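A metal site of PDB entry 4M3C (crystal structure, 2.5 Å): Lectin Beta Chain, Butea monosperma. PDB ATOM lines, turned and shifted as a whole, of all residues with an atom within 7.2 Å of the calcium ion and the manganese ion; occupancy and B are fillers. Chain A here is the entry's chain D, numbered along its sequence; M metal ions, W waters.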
ATOM      1  N   ASP A  88      21.620   1.753 -31.333  1.00  0.00           N
ATOM      2  CA  ASP A  88      22.090   0.393 -31.052  1.00  0.00           C
ATOM      3  C   ASP A  88      22.089   0.147 -29.542  1.00  0.00           C
ATOM      4  O   ASP A  88      22.109  -0.998 -29.104  1.00  0.00           O
ATOM      5  CB  ASP A  88      23.516   0.209 -31.594  1.00  0.00           C
ATOM      6  CG  ASP A  88      23.544  -0.167 -33.068  1.00  0.00           C
ATOM      7  OD1 ASP A  88      23.325  -1.352 -33.359  1.00  0.00           O
ATOM      8  OD2 ASP A  88      23.789   0.720 -33.921  1.00  0.00           O
ATOM      9  N   GLY A  89      22.068   1.242 -28.771  1.00  0.00           N
ATOM     10  CA  GLY A  89      21.870   1.149 -27.322  1.00  0.00           C
ATOM     11  C   GLY A  89      22.849   1.982 -26.513  1.00  0.00           C
ATOM     12  O   GLY A  89      23.537   2.839 -27.049  1.00  0.00           O
ATOM     13  N   ALA A 105      28.053   2.150 -33.925  1.00  0.00           N
ATOM     14  CA  ALA A 105      26.982   1.187 -34.161  1.00  0.00           C
ATOM     15  C   ALA A 105      26.870   0.290 -32.925  1.00  0.00           C
ATOM     16  O   ALA A 105      27.031   0.783 -31.800  1.00  0.00           O
ATOM     17  CB  ALA A 105      27.225   0.399 -35.442  1.00  0.00           C
ATOM     18  N   GLY A 106      26.625  -1.017 -33.127  1.00  0.00           N
ATOM     19  CA  GLY A 106      26.511  -2.002 -32.033  1.00  0.00           C
ATOM     20  C   GLY A 106      27.771  -2.421 -31.275  1.00  0.00           C
ATOM     21  O   GLY A 106      27.715  -3.287 -30.391  1.00  0.00           O
ATOM     22  N   PHE A 107      28.893  -1.816 -31.614  1.00  0.00           N
ATOM     23  CA  PHE A 107      30.056  -1.846 -30.722  1.00  0.00           C
ATOM     24  C   PHE A 107      29.919  -0.837 -29.562  1.00  0.00           C
ATOM     25  O   PHE A 107      30.653  -0.957 -28.581  1.00  0.00           O
ATOM     26  CB  PHE A 107      31.348  -1.539 -31.471  1.00  0.00           C
ATOM     27  CG  PHE A 107      31.572  -2.403 -32.665  1.00  0.00           C
ATOM     28  CD1 PHE A 107      32.144  -3.642 -32.521  1.00  0.00           C
ATOM     29  CD2 PHE A 107      31.200  -1.974 -33.922  1.00  0.00           C
ATOM     30  CE1 PHE A 107      32.326  -4.437 -33.615  1.00  0.00           C
ATOM     31  CE2 PHE A 107      31.382  -2.769 -35.016  1.00  0.00           C
ATOM     32  CZ  PHE A 107      31.959  -4.002 -34.865  1.00  0.00           C
ATOM     33  N   LEU A 108      29.010   0.128 -29.713  1.00  0.00           N
ATOM     34  CA  LEU A 108      28.633   1.050 -28.622  1.00  0.00           C
ATOM     35  C   LEU A 108      29.818   1.910 -28.159  1.00  0.00           C
ATOM     36  O   LEU A 108      29.976   2.203 -26.972  1.00  0.00           O
ATOM     37  CB  LEU A 108      27.937   0.292 -27.465  1.00  0.00           C
ATOM     38  CG  LEU A 108      26.733  -0.653 -27.766  1.00  0.00           C
ATOM     39  CD1 LEU A 108      26.353  -1.459 -26.537  1.00  0.00           C
ATOM     40  CD2 LEU A 108      25.500   0.080 -28.248  1.00  0.00           C
ATOM     41  N   GLU A 126      25.545  -3.017 -20.668  1.00  0.00           N
ATOM     42  CA  GLU A 126      24.887  -2.417 -21.862  1.00  0.00           C
ATOM     43  C   GLU A 126      23.359  -2.647 -21.860  1.00  0.00           C
ATOM     44  O   GLU A 126      22.835  -3.611 -21.296  1.00  0.00           O
ATOM     45  CB  GLU A 126      25.440  -3.027 -23.169  1.00  0.00           C
ATOM     46  CG  GLU A 126      25.249  -4.536 -23.176  1.00  0.00           C
ATOM     47  CD  GLU A 126      25.362  -5.210 -24.521  1.00  0.00           C
ATOM     48  OE1 GLU A 126      26.380  -4.967 -25.237  1.00  0.00           O
ATOM     49  OE2 GLU A 126      24.443  -6.036 -24.838  1.00  0.00           O
ATOM     50  N   PHE A 127      22.670  -1.719 -22.515  1.00  0.00           N
ATOM     51  CA  PHE A 127      21.230  -1.722 -22.657  1.00  0.00           C
ATOM     52  C   PHE A 127      21.096  -1.599 -24.146  1.00  0.00           C
ATOM     53  O   PHE A 127      21.205  -0.523 -24.725  1.00  0.00           O
ATOM     54  CB  PHE A 127      20.628  -0.525 -21.913  1.00  0.00           C
ATOM     55  CG  PHE A 127      20.978  -0.513 -20.459  1.00  0.00           C
ATOM     56  CD1 PHE A 127      20.147  -1.119 -19.525  1.00  0.00           C
ATOM     57  CD2 PHE A 127      22.139   0.082 -20.014  1.00  0.00           C
ATOM     58  CE1 PHE A 127      20.475  -1.107 -18.165  1.00  0.00           C
ATOM     59  CE2 PHE A 127      22.479   0.100 -18.670  1.00  0.00           C
ATOM     60  CZ  PHE A 127      21.648  -0.505 -17.736  1.00  0.00           C
ATOM     61  N   ASP A 128      20.852  -2.748 -24.756  1.00  0.00           N
ATOM     62  CA  ASP A 128      21.151  -3.002 -26.124  1.00  0.00           C
ATOM     63  C   ASP A 128      19.837  -3.122 -26.939  1.00  0.00           C
ATOM     64  O   ASP A 128      19.046  -4.065 -26.736  1.00  0.00           O
ATOM     65  CB  ASP A 128      22.006  -4.263 -26.131  1.00  0.00           C
ATOM     66  CG  ASP A 128      22.490  -4.645 -27.517  1.00  0.00           C
ATOM     67  OD1 ASP A 128      23.312  -5.621 -27.606  1.00  0.00           O
ATOM     68  OD2 ASP A 128      22.056  -3.994 -28.511  1.00  0.00           O
ATOM     69  N   THR A 129      19.625  -2.158 -27.852  1.00  0.00           N
ATOM     70  CA  THR A 129      18.358  -2.015 -28.568  1.00  0.00           C
ATOM     71  C   THR A 129      18.242  -2.651 -29.951  1.00  0.00           C
ATOM     72  O   THR A 129      17.148  -2.670 -30.562  1.00  0.00           O
ATOM     73  CB  THR A 129      17.877  -0.561 -28.638  1.00  0.00           C
ATOM     74  OG1 THR A 129      18.871   0.258 -29.249  1.00  0.00           O
ATOM     75  CG2 THR A 129      17.493  -0.059 -27.209  1.00  0.00           C
ATOM     76  N   TYR A 130      19.352  -3.231 -30.415  1.00  0.00           N
ATOM     77  CA  TYR A 130      19.372  -3.841 -31.726  1.00  0.00           C
ATOM     78  C   TYR A 130      20.112  -5.175 -31.795  1.00  0.00           C
ATOM     79  O   TYR A 130      21.268  -5.306 -31.367  1.00  0.00           O
ATOM     80  CB  TYR A 130      19.921  -2.874 -32.766  1.00  0.00           C
ATOM     81  CG  TYR A 130      19.993  -3.460 -34.159  1.00  0.00           C
ATOM     82  CD1 TYR A 130      19.073  -3.114 -35.151  1.00  0.00           C
ATOM     83  CD2 TYR A 130      20.961  -4.406 -34.481  1.00  0.00           C
ATOM     84  CE1 TYR A 130      19.138  -3.648 -36.411  1.00  0.00           C
ATOM     85  CE2 TYR A 130      21.034  -4.971 -35.734  1.00  0.00           C
ATOM     86  CZ  TYR A 130      20.128  -4.581 -36.698  1.00  0.00           C
ATOM     87  OH  TYR A 130      20.231  -5.159 -37.948  1.00  0.00           O
ATOM     88  N   GLU A 131      19.455  -6.164 -32.387  1.00  0.00           N
ATOM     89  CA  GLU A 131      19.996  -7.483 -32.414  1.00  0.00           C
ATOM     90  C   GLU A 131      21.083  -7.599 -33.430  1.00  0.00           C
ATOM     91  O   GLU A 131      20.811  -7.552 -34.633  1.00  0.00           O
ATOM     92  CB  GLU A 131      18.916  -8.465 -32.755  1.00  0.00           C
ATOM     93  CG  GLU A 131      19.340  -9.850 -32.412  1.00  0.00           C
ATOM     94  CD  GLU A 131      18.489 -10.853 -33.102  1.00  0.00           C
ATOM     95  OE1 GLU A 131      17.521 -10.407 -33.776  1.00  0.00           O
ATOM     96  OE2 GLU A 131      18.786 -12.050 -32.975  1.00  0.00           O
ATOM     97  N   ASN A 132      22.325  -7.725 -32.949  1.00  0.00           N
ATOM     98  CA  ASN A 132      23.473  -7.989 -33.795  1.00  0.00           C
ATOM     99  C   ASN A 132      23.787  -9.477 -33.666  1.00  0.00           C
ATOM    100  O   ASN A 132      24.541  -9.897 -32.788  1.00  0.00           O
ATOM    101  CB  ASN A 132      24.685  -7.159 -33.389  1.00  0.00           C
ATOM    102  CG  ASN A 132      24.433  -5.663 -33.482  1.00  0.00           C
ATOM    103  OD1 ASN A 132      23.752  -5.083 -32.635  1.00  0.00           O
ATOM    104  ND2 ASN A 132      25.042  -5.020 -34.474  1.00  0.00           N
ATOM    105  N   THR A 133      23.165 -10.253 -34.553  1.00  0.00           N
ATOM    106  CA  THR A 133      23.376 -11.710 -34.658  1.00  0.00           C
ATOM    107  C   THR A 133      24.884 -12.065 -34.750  1.00  0.00           C
ATOM    108  O   THR A 133      25.327 -13.084 -34.222  1.00  0.00           O
ATOM    109  CB  THR A 133      22.555 -12.324 -35.838  1.00  0.00           C
ATOM    110  OG1 THR A 133      23.425 -13.010 -36.743  1.00  0.00           O
ATOM    111  CG2 THR A 133      21.833 -11.246 -36.641  1.00  0.00           C
ATOM    112  N   PHE A 135      27.113 -10.777 -33.002  1.00  0.00           N
ATOM    113  CA  PHE A 135      27.680 -10.637 -31.675  1.00  0.00           C
ATOM    114  C   PHE A 135      27.047 -11.625 -30.706  1.00  0.00           C
ATOM    115  O   PHE A 135      27.273 -11.525 -29.506  1.00  0.00           O
ATOM    116  CB  PHE A 135      27.442  -9.232 -31.127  1.00  0.00           C
ATOM    117  CG  PHE A 135      28.085  -8.128 -31.925  1.00  0.00           C
ATOM    118  CD1 PHE A 135      29.208  -8.363 -32.726  1.00  0.00           C
ATOM    119  CD2 PHE A 135      27.608  -6.829 -31.818  1.00  0.00           C
ATOM    120  CE1 PHE A 135      29.815  -7.325 -33.446  1.00  0.00           C
ATOM    121  CE2 PHE A 135      28.191  -5.782 -32.527  1.00  0.00           C
ATOM    122  CZ  PHE A 135      29.298  -6.035 -33.347  1.00  0.00           C
ATOM    123  N   LEU A 136      26.257 -12.552 -31.229  1.00  0.00           N
ATOM    124  CA  LEU A 136      25.534 -13.547 -30.421  1.00  0.00           C
ATOM    125  C   LEU A 136      24.377 -12.942 -29.617  1.00  0.00           C
ATOM    126  O   LEU A 136      23.930 -13.523 -28.610  1.00  0.00           O
ATOM    127  CB  LEU A 136      26.497 -14.341 -29.509  1.00  0.00           C
ATOM    128  CG  LEU A 136      27.039 -15.728 -29.942  1.00  0.00           C
ATOM    129  CD1 LEU A 136      27.774 -15.703 -31.295  1.00  0.00           C
ATOM    130  CD2 LEU A 136      27.901 -16.378 -28.840  1.00  0.00           C
ATOM    131  N   ASP A 137      23.875 -11.795 -30.072  1.00  0.00           N
ATOM    132  CA  ASP A 137      22.738 -11.118 -29.435  1.00  0.00           C
ATOM    133  C   ASP A 137      21.485 -11.954 -29.493  1.00  0.00           C
ATOM    134  O   ASP A 137      21.131 -12.435 -30.548  1.00  0.00           O
ATOM    135  CB  ASP A 137      22.402  -9.812 -30.148  1.00  0.00           C
ATOM    136  CG  ASP A 137      23.153  -8.617 -29.588  1.00  0.00           C
ATOM    137  OD1 ASP A 137      23.276  -7.608 -30.326  1.00  0.00           O
ATOM    138  OD2 ASP A 137      23.595  -8.675 -28.420  1.00  0.00           O
ATOM    139  N   PRO A 138      20.794 -12.103 -28.367  1.00  0.00           N
ATOM    140  CA  PRO A 138      19.482 -12.733 -28.297  1.00  0.00           C
ATOM    141  C   PRO A 138      18.396 -12.019 -29.109  1.00  0.00           C
ATOM    142  O   PRO A 138      18.482 -10.801 -29.335  1.00  0.00           O
ATOM    143  CB  PRO A 138      19.136 -12.650 -26.809  1.00  0.00           C
ATOM    144  CG  PRO A 138      19.909 -11.492 -26.313  1.00  0.00           C
ATOM    145  CD  PRO A 138      21.207 -11.555 -27.071  1.00  0.00           C
ATOM    146  N   ASP A 140      15.790 -10.560 -28.574  1.00  0.00           N
ATOM    147  CA  ASP A 140      15.018  -9.537 -27.894  1.00  0.00           C
ATOM    148  C   ASP A 140      15.971  -8.451 -27.449  1.00  0.00           C
ATOM    149  O   ASP A 140      17.165  -8.727 -27.207  1.00  0.00           O
ATOM    150  CB  ASP A 140      14.213 -10.106 -26.677  1.00  0.00           C
ATOM    151  CG  ASP A 140      14.992 -11.182 -25.844  1.00  0.00           C
ATOM    152  OD1 ASP A 140      14.769 -12.392 -26.109  1.00  0.00           O
ATOM    153  OD2 ASP A 140      15.806 -10.856 -24.901  1.00  0.00           O
ATOM    154  N   HIS A 142      17.781  -6.209 -24.720  1.00  0.00           N
ATOM    155  CA  HIS A 142      18.355  -6.847 -23.500  1.00  0.00           C
ATOM    156  C   HIS A 142      19.261  -5.969 -22.689  1.00  0.00           C
ATOM    157  O   HIS A 142      19.651  -4.885 -23.108  1.00  0.00           O
ATOM    158  CB  HIS A 142      19.092  -8.145 -23.858  1.00  0.00           C
ATOM    159  CG  HIS A 142      20.073  -7.992 -24.990  1.00  0.00           C
ATOM    160  ND1 HIS A 142      19.701  -7.992 -26.259  1.00  0.00           N
ATOM    161  CD2 HIS A 142      21.436  -7.727 -24.983  1.00  0.00           C
ATOM    162  CE1 HIS A 142      20.761  -7.745 -27.047  1.00  0.00           C
ATOM    163  NE2 HIS A 142      21.824  -7.592 -26.262  1.00  0.00           N
ATOM    164  N   ILE A 143      19.575  -6.463 -21.501  1.00  0.00           N
ATOM    165  CA  ILE A 143      20.606  -5.933 -20.642  1.00  0.00           C
ATOM    166  C   ILE A 143      21.716  -6.971 -20.673  1.00  0.00           C
ATOM    167  O   ILE A 143      21.446  -8.171 -20.615  1.00  0.00           O
ATOM    168  CB  ILE A 143      20.084  -5.734 -19.213  1.00  0.00           C
ATOM    169  CG1 ILE A 143      19.050  -4.613 -19.212  1.00  0.00           C
ATOM    170  CG2 ILE A 143      21.213  -5.356 -18.277  1.00  0.00           C
ATOM    171  CD1 ILE A 143      18.283  -4.508 -17.924  1.00  0.00           C
ATOM    172  N   GLY A 144      22.959  -6.489 -20.787  1.00  0.00           N
ATOM    173  CA  GLY A 144      24.070  -7.368 -20.936  1.00  0.00           C
ATOM    174  C   GLY A 144      25.271  -6.922 -20.142  1.00  0.00           C
ATOM    175  O   GLY A 144      25.519  -5.725 -19.968  1.00  0.00           O
ATOM    176  N   ASP A 146      29.187  -6.972 -20.257  1.00  0.00           N
ATOM    177  CA  ASP A 146      30.278  -7.055 -21.257  1.00  0.00           C
ATOM    178  C   ASP A 146      31.638  -6.966 -20.629  1.00  0.00           C
ATOM    179  O   ASP A 146      32.070  -5.869 -20.241  1.00  0.00           O
ATOM    180  CB  ASP A 146      30.183  -5.880 -22.210  1.00  0.00           C
ATOM    181  CG  ASP A 146      29.051  -6.001 -23.177  1.00  0.00           C
ATOM    182  OD1 ASP A 146      28.450  -7.090 -23.205  1.00  0.00           O
ATOM    183  OD2 ASP A 146      28.723  -5.008 -23.891  1.00  0.00           O
ATOM    184  N   ILE A 150      32.044  -7.351 -26.741  1.00  0.00           N
ATOM    185  CA  ILE A 150      30.629  -6.988 -27.009  1.00  0.00           C
ATOM    186  C   ILE A 150      29.698  -8.229 -27.002  1.00  0.00           C
ATOM    187  O   ILE A 150      28.482  -8.095 -26.977  1.00  0.00           O
ATOM    188  CB  ILE A 150      30.479  -6.199 -28.325  1.00  0.00           C
ATOM    189  CG1 ILE A 150      29.083  -5.596 -28.431  1.00  0.00           C
ATOM    190  CG2 ILE A 150      30.819  -7.064 -29.551  1.00  0.00           C
ATOM    191  CD1 ILE A 150      28.867  -4.418 -27.511  1.00  0.00           C
ATOM    192  N   LYS A 151      30.298  -9.417 -27.026  1.00  0.00           N
ATOM    193  CA  LYS A 151      29.586 -10.662 -26.975  1.00  0.00           C
ATOM    194  C   LYS A 151      29.471 -10.938 -25.470  1.00  0.00           C
ATOM    195  O   LYS A 151      30.376 -11.519 -24.857  1.00  0.00           O
ATOM    196  CB  LYS A 151      30.414 -11.716 -27.705  1.00  0.00           C
ATOM    197  CG  LYS A 151      29.732 -13.031 -28.064  1.00  0.00           C
ATOM    198  CD  LYS A 151      30.634 -13.892 -28.976  1.00  0.00           C
ATOM    199  CE  LYS A 151      30.839 -13.317 -30.387  1.00  0.00           C
ATOM    200  NZ  LYS A 151      32.190 -13.638 -30.961  1.00  0.00           N
ATOM    201  N   SER A 152      28.336 -10.490 -24.908  1.00  0.00           N
ATOM    202  CA  SER A 152      28.059 -10.456 -23.480  1.00  0.00           C
ATOM    203  C   SER A 152      28.265 -11.795 -22.836  1.00  0.00           C
ATOM    204  O   SER A 152      27.769 -12.789 -23.349  1.00  0.00           O
ATOM    205  CB  SER A 152      26.580 -10.054 -23.230  1.00  0.00           C
ATOM    206  OG  SER A 152      26.249  -8.737 -23.635  1.00  0.00           O
ATOM    207  N   THR A 155      23.347 -12.095 -20.480  1.00  0.00           N
ATOM    208  CA  THR A 155      22.302 -11.088 -20.701  1.00  0.00           C
ATOM    209  C   THR A 155      20.958 -11.512 -20.089  1.00  0.00           C
ATOM    210  O   THR A 155      20.803 -12.638 -19.618  1.00  0.00           O
ATOM    211  CB  THR A 155      21.901 -11.033 -22.193  1.00  0.00           C
ATOM    212  OG1 THR A 155      21.476 -12.352 -22.586  1.00  0.00           O
ATOM    213  CG2 THR A 155      23.022 -10.575 -23.101  1.00  0.00           C
HETATM  214 CA    CA M   1      23.469  -5.089 -30.390  1.00  0.00          CA
HETATM  215 MN    MN M   2      24.195  -7.435 -26.726  1.00  0.00          MN
HETATM  216  O   HOH W   1      23.136  -2.912 -30.639  1.00  0.00           O
HETATM  217  O   HOH W   2      26.445  -6.435 -27.468  1.00  0.00           O
HETATM  218  O   HOH W   3      25.841  -4.948 -29.564  1.00  0.00           O
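A ring nitrogen (ND1) of His 142 is in hydrogen-bond range of the backbone carbonyl oxygen (O) of Asp 140 (2.8 Å).
OG of Ser 152 is in hydrogen-bond range of OD1 of Asp 146, at 2.8 Å.
The backbone NH (N) of Glu 126 sits at hydrogen-bond distance from the backbone carbonyl oxygen (O) of Gly 144 (2.8 Å).
OE2 of Glu 126 sits close to OG of Ser 152, at 3.5 Å.
OD2 of Asp 146 sits close to OE1 of Glu 126 (2.7 Å).
Of the 27 residues printed, 4 come within 4 Å of the calcium ion.
The nearest printed residue that does not touch the calcium ion is Asp 88 (4.5 Å).
OG of Ser 152 touches the manganese ion (3.9 Å).
The nearest printed residue that does not touch the manganese ion is Ile 150 (4.3 Å).
Water W1 is bound to the calcium ion.
OD1 of Asn 132 is bound to the calcium ion (2.3 Å).
O of Tyr 130 is bound to the calcium ion, 2.4 Å away.
The calcium ion is bound by water W3 (2.5 Å).
The side-chain carboxylate (OD1) of Asp 137 binds the calcium ion (2.5 Å).
OD2 of Asp 128 binds the calcium ion, 2.6 Å away.
OD1 of Asp 128 is bound to the calcium ion, 2.8 Å away.
The manganese ion is bound by OD2 of Asp 137 (2.2 Å), OD1 of Asp 128 (2.2 Å), OE2 of Glu 126 (2.4 Å), NE2 of His 142 (2.4 Å) and water W2 (2.6 Å).
The manganese ion has five donor atoms within binding distance.
Water W2 lies within hydrogen-bond range of OE1 of Glu 126 (2.7 Å) and O of Ile 150 (2.7 Å).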
